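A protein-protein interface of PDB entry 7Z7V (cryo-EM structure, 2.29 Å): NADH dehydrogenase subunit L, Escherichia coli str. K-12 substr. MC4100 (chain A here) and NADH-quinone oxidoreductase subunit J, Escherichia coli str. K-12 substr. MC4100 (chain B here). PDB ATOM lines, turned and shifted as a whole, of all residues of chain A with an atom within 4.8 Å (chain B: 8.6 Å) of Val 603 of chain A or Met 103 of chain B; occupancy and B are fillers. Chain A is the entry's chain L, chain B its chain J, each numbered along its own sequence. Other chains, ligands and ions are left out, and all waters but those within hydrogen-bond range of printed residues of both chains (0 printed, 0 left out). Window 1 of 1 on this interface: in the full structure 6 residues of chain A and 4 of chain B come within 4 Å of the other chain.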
ATOM      1  N   SER A 599      -1.179  14.020   2.392  1.00  0.00           N
ATOM      2  CA  SER A 599      -1.578  12.859   1.598  1.00  0.00           C
ATOM      3  C   SER A 599      -1.137  11.544   2.238  1.00  0.00           C
ATOM      4  O   SER A 599      -1.844  10.536   2.126  1.00  0.00           O
ATOM      5  CB  SER A 599      -1.032  12.971   0.177  1.00  0.00           C
ATOM      6  OG  SER A 599       0.322  13.367   0.176  1.00  0.00           O
ATOM      7  N   ILE A 600       0.016  11.536   2.915  1.00  0.00           N
ATOM      8  CA  ILE A 600       0.454  10.359   3.663  1.00  0.00           C
ATOM      9  C   ILE A 600      -0.527  10.053   4.787  1.00  0.00           C
ATOM     10  O   ILE A 600      -0.912   8.897   4.997  1.00  0.00           O
ATOM     11  CB  ILE A 600       1.883  10.572   4.203  1.00  0.00           C
ATOM     12  CG1 ILE A 600       2.921  10.329   3.113  1.00  0.00           C
ATOM     13  CG2 ILE A 600       2.178   9.649   5.373  1.00  0.00           C
ATOM     14  CD1 ILE A 600       4.266  10.935   3.418  1.00  0.00           C
ATOM     15  N   GLY A 601      -0.951  11.088   5.518  1.00  0.00           N
ATOM     16  CA  GLY A 601      -1.948  10.900   6.554  1.00  0.00           C
ATOM     17  C   GLY A 601      -3.288  10.451   6.015  1.00  0.00           C
ATOM     18  O   GLY A 601      -3.986   9.669   6.661  1.00  0.00           O
ATOM     19  N   ALA A 602      -3.659  10.930   4.825  1.00  0.00           N
ATOM     20  CA  ALA A 602      -4.868  10.445   4.171  1.00  0.00           C
ATOM     21  C   ALA A 602      -4.768   8.960   3.855  1.00  0.00           C
ATOM     22  O   ALA A 602      -5.712   8.201   4.102  1.00  0.00           O
ATOM     23  CB  ALA A 602      -5.132  11.246   2.895  1.00  0.00           C
ATOM     24  N   VAL A 603      -3.616   8.532   3.335  1.00  0.00           N
ATOM     25  CA  VAL A 603      -3.392   7.121   3.028  1.00  0.00           C
ATOM     26  C   VAL A 603      -3.458   6.277   4.296  1.00  0.00           C
ATOM     27  O   VAL A 603      -4.097   5.219   4.323  1.00  0.00           O
ATOM     28  CB  VAL A 603      -2.046   6.955   2.296  1.00  0.00           C
ATOM     29  CG1 VAL A 603      -1.526   5.530   2.407  1.00  0.00           C
ATOM     30  CG2 VAL A 603      -2.184   7.364   0.845  1.00  0.00           C
ATOM     31  N   VAL A 604      -2.823   6.750   5.371  1.00  0.00           N
ATOM     32  CA  VAL A 604      -2.794   6.007   6.629  1.00  0.00           C
ATOM     33  C   VAL A 604      -4.191   5.904   7.235  1.00  0.00           C
ATOM     34  O   VAL A 604      -4.604   4.828   7.684  1.00  0.00           O
ATOM     35  CB  VAL A 604      -1.790   6.659   7.599  1.00  0.00           C
ATOM     36  CG1 VAL A 604      -1.983   6.145   9.016  1.00  0.00           C
ATOM     37  CG2 VAL A 604      -0.371   6.398   7.135  1.00  0.00           C
ATOM     38  N   VAL A 605      -4.949   7.005   7.231  1.00  0.00           N
ATOM     39  CA  VAL A 605      -6.302   7.003   7.785  1.00  0.00           C
ATOM     40  C   VAL A 605      -7.213   6.080   6.981  1.00  0.00           C
ATOM     41  O   VAL A 605      -7.972   5.285   7.551  1.00  0.00           O
ATOM     42  CB  VAL A 605      -6.849   8.444   7.846  1.00  0.00           C
ATOM     43  CG1 VAL A 605      -8.370   8.467   7.863  1.00  0.00           C
ATOM     44  CG2 VAL A 605      -6.300   9.164   9.062  1.00  0.00           C
ATOM     45  N   LEU A 606      -7.127   6.146   5.649  1.00  0.00           N
ATOM     46  CA  LEU A 606      -7.958   5.296   4.803  1.00  0.00           C
ATOM     47  C   LEU A 606      -7.607   3.821   4.968  1.00  0.00           C
ATOM     48  O   LEU A 606      -8.503   2.972   5.047  1.00  0.00           O
ATOM     49  CB  LEU A 606      -7.813   5.722   3.344  1.00  0.00           C
ATOM     50  CG  LEU A 606      -8.531   6.996   2.906  1.00  0.00           C
ATOM     51  CD1 LEU A 606      -7.904   7.544   1.639  1.00  0.00           C
ATOM     52  CD2 LEU A 606      -9.998   6.722   2.697  1.00  0.00           C
ATOM     53  N   ALA A 607      -6.311   3.500   5.037  1.00  0.00           N
ATOM     54  CA  ALA A 607      -5.890   2.115   5.217  1.00  0.00           C
ATOM     55  C   ALA A 607      -6.310   1.580   6.579  1.00  0.00           C
ATOM     56  O   ALA A 607      -6.731   0.423   6.691  1.00  0.00           O
ATOM     57  CB  ALA A 607      -4.379   2.000   5.039  1.00  0.00           C
ATOM     58  N   PRO B  96       5.683  10.264  -4.722  1.00  0.00           N
ATOM     59  CA  PRO B  96       4.287  10.717  -4.832  1.00  0.00           C
ATOM     60  C   PRO B  96       3.419   9.872  -5.750  1.00  0.00           C
ATOM     61  O   PRO B  96       2.220   9.744  -5.483  1.00  0.00           O
ATOM     62  CB  PRO B  96       4.432  12.145  -5.363  1.00  0.00           C
ATOM     63  CG  PRO B  96       5.742  12.592  -4.866  1.00  0.00           C
ATOM     64  CD  PRO B  96       6.627  11.394  -4.819  1.00  0.00           C
ATOM     65  N   ALA B  97       3.978   9.292  -6.817  1.00  0.00           N
ATOM     66  CA  ALA B  97       3.182   8.415  -7.674  1.00  0.00           C
ATOM     67  C   ALA B  97       2.753   7.154  -6.936  1.00  0.00           C
ATOM     68  O   ALA B  97       1.604   6.722  -7.064  1.00  0.00           O
ATOM     69  CB  ALA B  97       3.954   8.053  -8.939  1.00  0.00           C
ATOM     70  N   ILE B  98       3.659   6.557  -6.155  1.00  0.00           N
ATOM     71  CA  ILE B  98       3.299   5.393  -5.348  1.00  0.00           C
ATOM     72  C   ILE B  98       2.264   5.771  -4.296  1.00  0.00           C
ATOM     73  O   ILE B  98       1.304   5.028  -4.057  1.00  0.00           O
ATOM     74  CB  ILE B  98       4.559   4.762  -4.717  1.00  0.00           C
ATOM     75  CG1 ILE B  98       5.404   4.059  -5.779  1.00  0.00           C
ATOM     76  CG2 ILE B  98       4.205   3.780  -3.613  1.00  0.00           C
ATOM     77  CD1 ILE B  98       6.858   3.903  -5.396  1.00  0.00           C
ATOM     78  N   LEU B  99       2.427   6.941  -3.673  1.00  0.00           N
ATOM     79  CA  LEU B  99       1.475   7.396  -2.660  1.00  0.00           C
ATOM     80  C   LEU B  99       0.081   7.599  -3.251  1.00  0.00           C
ATOM     81  O   LEU B  99      -0.925   7.156  -2.678  1.00  0.00           O
ATOM     82  CB  LEU B  99       1.988   8.689  -2.035  1.00  0.00           C
ATOM     83  CG  LEU B  99       1.327   9.190  -0.759  1.00  0.00           C
ATOM     84  CD1 LEU B  99       1.509   8.190   0.363  1.00  0.00           C
ATOM     85  CD2 LEU B  99       1.926  10.531  -0.397  1.00  0.00           C
ATOM     86  N   SER B 100       0.009   8.245  -4.417  1.00  0.00           N
ATOM     87  CA  SER B 100      -1.274   8.467  -5.073  1.00  0.00           C
ATOM     88  C   SER B 100      -1.875   7.163  -5.575  1.00  0.00           C
ATOM     89  O   SER B 100      -3.098   6.997  -5.553  1.00  0.00           O
ATOM     90  CB  SER B 100      -1.112   9.453  -6.223  1.00  0.00           C
ATOM     91  OG  SER B 100      -0.386  10.598  -5.816  1.00  0.00           O
ATOM     92  N   ALA B 101      -1.037   6.226  -6.025  1.00  0.00           N
ATOM     93  CA  ALA B 101      -1.539   4.926  -6.455  1.00  0.00           C
ATOM     94  C   ALA B 101      -2.110   4.136  -5.285  1.00  0.00           C
ATOM     95  O   ALA B 101      -3.132   3.462  -5.432  1.00  0.00           O
ATOM     96  CB  ALA B 101      -0.429   4.136  -7.146  1.00  0.00           C
ATOM     97  N   ILE B 102      -1.467   4.211  -4.117  1.00  0.00           N
ATOM     98  CA  ILE B 102      -1.987   3.542  -2.928  1.00  0.00           C
ATOM     99  C   ILE B 102      -3.315   4.158  -2.505  1.00  0.00           C
ATOM    100  O   ILE B 102      -4.276   3.441  -2.186  1.00  0.00           O
ATOM    101  CB  ILE B 102      -0.950   3.592  -1.790  1.00  0.00           C
ATOM    102  CG1 ILE B 102       0.234   2.681  -2.101  1.00  0.00           C
ATOM    103  CG2 ILE B 102      -1.565   3.167  -0.472  1.00  0.00           C
ATOM    104  CD1 ILE B 102       1.432   2.946  -1.227  1.00  0.00           C
ATOM    105  N   MET B 103      -3.396   5.494  -2.511  1.00  0.00           N
ATOM    106  CA  MET B 103      -4.650   6.163  -2.174  1.00  0.00           C
ATOM    107  C   MET B 103      -5.752   5.808  -3.165  1.00  0.00           C
ATOM    108  O   MET B 103      -6.899   5.568  -2.768  1.00  0.00           O
ATOM    109  CB  MET B 103      -4.444   7.675  -2.119  1.00  0.00           C
ATOM    110  CG  MET B 103      -5.644   8.439  -1.586  1.00  0.00           C
ATOM    111  SD  MET B 103      -5.406  10.222  -1.618  1.00  0.00           S
ATOM    112  CE  MET B 103      -3.830  10.351  -0.784  1.00  0.00           C
ATOM    113  N   LEU B 104      -5.413   5.744  -4.453  1.00  0.00           N
ATOM    114  CA  LEU B 104      -6.379   5.366  -5.475  1.00  0.00           C
ATOM    115  C   LEU B 104      -6.839   3.927  -5.300  1.00  0.00           C
ATOM    116  O   LEU B 104      -8.019   3.629  -5.486  1.00  0.00           O
ATOM    117  CB  LEU B 104      -5.771   5.572  -6.861  1.00  0.00           C
ATOM    118  CG  LEU B 104      -6.684   5.325  -8.059  1.00  0.00           C
ATOM    119  CD1 LEU B 104      -7.877   6.256  -8.009  1.00  0.00           C
ATOM    120  CD2 LEU B 104      -5.914   5.505  -9.350  1.00  0.00           C
ATOM    121  N   VAL B 105      -5.924   3.025  -4.938  1.00  0.00           N
ATOM    122  CA  VAL B 105      -6.281   1.624  -4.730  1.00  0.00           C
ATOM    123  C   VAL B 105      -7.235   1.484  -3.550  1.00  0.00           C
ATOM    124  O   VAL B 105      -8.243   0.770  -3.632  1.00  0.00           O
ATOM    125  CB  VAL B 105      -5.005   0.777  -4.552  1.00  0.00           C
ATOM    126  CG1 VAL B 105      -5.284  -0.499  -3.770  1.00  0.00           C
ATOM    127  CG2 VAL B 105      -4.402   0.442  -5.903  1.00  0.00           C
ATOM    128  N   VAL B 106      -6.953   2.189  -2.451  1.00  0.00           N
ATOM    129  CA  VAL B 106      -7.823   2.120  -1.277  1.00  0.00           C
ATOM    130  C   VAL B 106      -9.199   2.714  -1.578  1.00  0.00           C
ATOM    131  O   VAL B 106     -10.235   2.124  -1.234  1.00  0.00           O
ATOM    132  CB  VAL B 106      -7.152   2.814  -0.078  1.00  0.00           C
ATOM    133  CG1 VAL B 106      -8.102   2.877   1.093  1.00  0.00           C
ATOM    134  CG2 VAL B 106      -5.889   2.077   0.318  1.00  0.00           C
ATOM    135  N   ILE B 107      -9.234   3.867  -2.255  1.00  0.00           N
ATOM    136  CA  ILE B 107     -10.503   4.512  -2.576  1.00  0.00           C
ATOM    137  C   ILE B 107     -11.305   3.668  -3.564  1.00  0.00           C
ATOM    138  O   ILE B 107     -12.525   3.537  -3.434  1.00  0.00           O
ATOM    139  CB  ILE B 107     -10.248   5.941  -3.097  1.00  0.00           C
ATOM    140  CG1 ILE B 107      -9.774   6.842  -1.956  1.00  0.00           C
ATOM    141  CG2 ILE B 107     -11.495   6.546  -3.707  1.00  0.00           C
ATOM    142  CD1 ILE B 107      -9.283   8.192  -2.413  1.00  0.00           C
ATOM    143  N   VAL B 108     -10.631   3.047  -4.535  1.00  0.00           N
ATOM    144  CA  VAL B 108     -11.310   2.197  -5.508  1.00  0.00           C
ATOM    145  C   VAL B 108     -11.860   0.942  -4.837  1.00  0.00           C
ATOM    146  O   VAL B 108     -12.973   0.501  -5.146  1.00  0.00           O
ATOM    147  CB  VAL B 108     -10.351   1.873  -6.672  1.00  0.00           C
ATOM    148  CG1 VAL B 108     -10.688   0.547  -7.340  1.00  0.00           C
ATOM    149  CG2 VAL B 108     -10.372   2.993  -7.695  1.00  0.00           C
ATOM    150  N   TYR B 109     -11.109   0.367  -3.892  1.00  0.00           N
ATOM    151  CA  TYR B 109     -11.608  -0.795  -3.162  1.00  0.00           C
ATOM    152  C   TYR B 109     -12.830  -0.433  -2.329  1.00  0.00           C
ATOM    153  O   TYR B 109     -13.761  -1.235  -2.201  1.00  0.00           O
ATOM    154  CB  TYR B 109     -10.484  -1.399  -2.304  1.00  0.00           C
ATOM    155  CG  TYR B 109     -10.905  -2.326  -1.166  1.00  0.00           C
ATOM    156  CD1 TYR B 109     -11.279  -1.834   0.087  1.00  0.00           C
ATOM    157  CD2 TYR B 109     -10.957  -3.700  -1.364  1.00  0.00           C
ATOM    158  CE1 TYR B 109     -11.669  -2.681   1.101  1.00  0.00           C
ATOM    159  CE2 TYR B 109     -11.346  -4.553  -0.352  1.00  0.00           C
ATOM    160  CZ  TYR B 109     -11.701  -4.040   0.875  1.00  0.00           C
ATOM    161  OH  TYR B 109     -12.089  -4.889   1.885  1.00  0.00           O
ATOM    162  N   ALA B 110     -12.836   0.764  -1.741  1.00  0.00           N
ATOM    163  CA  ALA B 110     -14.026   1.216  -1.026  1.00  0.00           C
ATOM    164  C   ALA B 110     -15.191   1.455  -1.980  1.00  0.00           C
ATOM    165  O   ALA B 110     -16.348   1.193  -1.631  1.00  0.00           O
ATOM    166  CB  ALA B 110     -13.714   2.481  -0.237  1.00  0.00           C
ATOM    167  N   ILE B 111     -14.903   1.962  -3.181  1.00  0.00           N
ATOM    168  CA  ILE B 111     -15.946   2.253  -4.162  1.00  0.00           C
ATOM    169  C   ILE B 111     -16.606   0.967  -4.649  1.00  0.00           C
ATOM    170  O   ILE B 111     -17.836   0.887  -4.748  1.00  0.00           O
ATOM    171  CB  ILE B 111     -15.350   3.068  -5.328  1.00  0.00           C
ATOM    172  CG1 ILE B 111     -15.250   4.546  -4.960  1.00  0.00           C
ATOM    173  CG2 ILE B 111     -16.180   2.926  -6.589  1.00  0.00           C
ATOM    174  CD1 ILE B 111     -14.295   5.314  -5.834  1.00  0.00           C
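Among the printed residues, pairs that only touch across the chains: Ser 599 of chain A with Leu 99 of chain B, Ser 599 of chain A with Met 103 of chain B, Leu 606 of chain A with Val 106 of chain B, Ile 600 of chain A with Leu 99 of chain B, Val 603 of chain A with Ile 102 of chain B, Val 603 of chain A with Met 103 of chain B and Val 603 of chain A with Leu 99 of chain B.
Val 603 of chain A touches three residues of chain B. Printed residues of chain A within 4 Å of Met 103 of chain B: Ser 599 and Val 603. Of the printed residues of chain B, Ile 600 of chain A touches Leu 99 (3.7 Å). Printed residues of chain A within 4 Å of Ile 102 of chain B: Val 603 (3.7 Å). Ile 98 of chain B touches none of the printed residues of chain A. Pro 96 of chain B touches none of the printed residues of chain A. The nearest printed residue of chain A that does not touch Leu 99 of chain B is Gly 601 of chain A (6.4 Å).
Of the 16 printed residues of chain B, 4 touch a printed residue of chain A. Of the 9 printed residues of chain A, 4 touch a printed residue of chain B. Among the printed residues, 7 pairs touch across the chains. Among the printed residues, no Asp or Glu carboxylate lies within 4 Å of a Lys or Arg side-chain nitrogen of the other chain.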
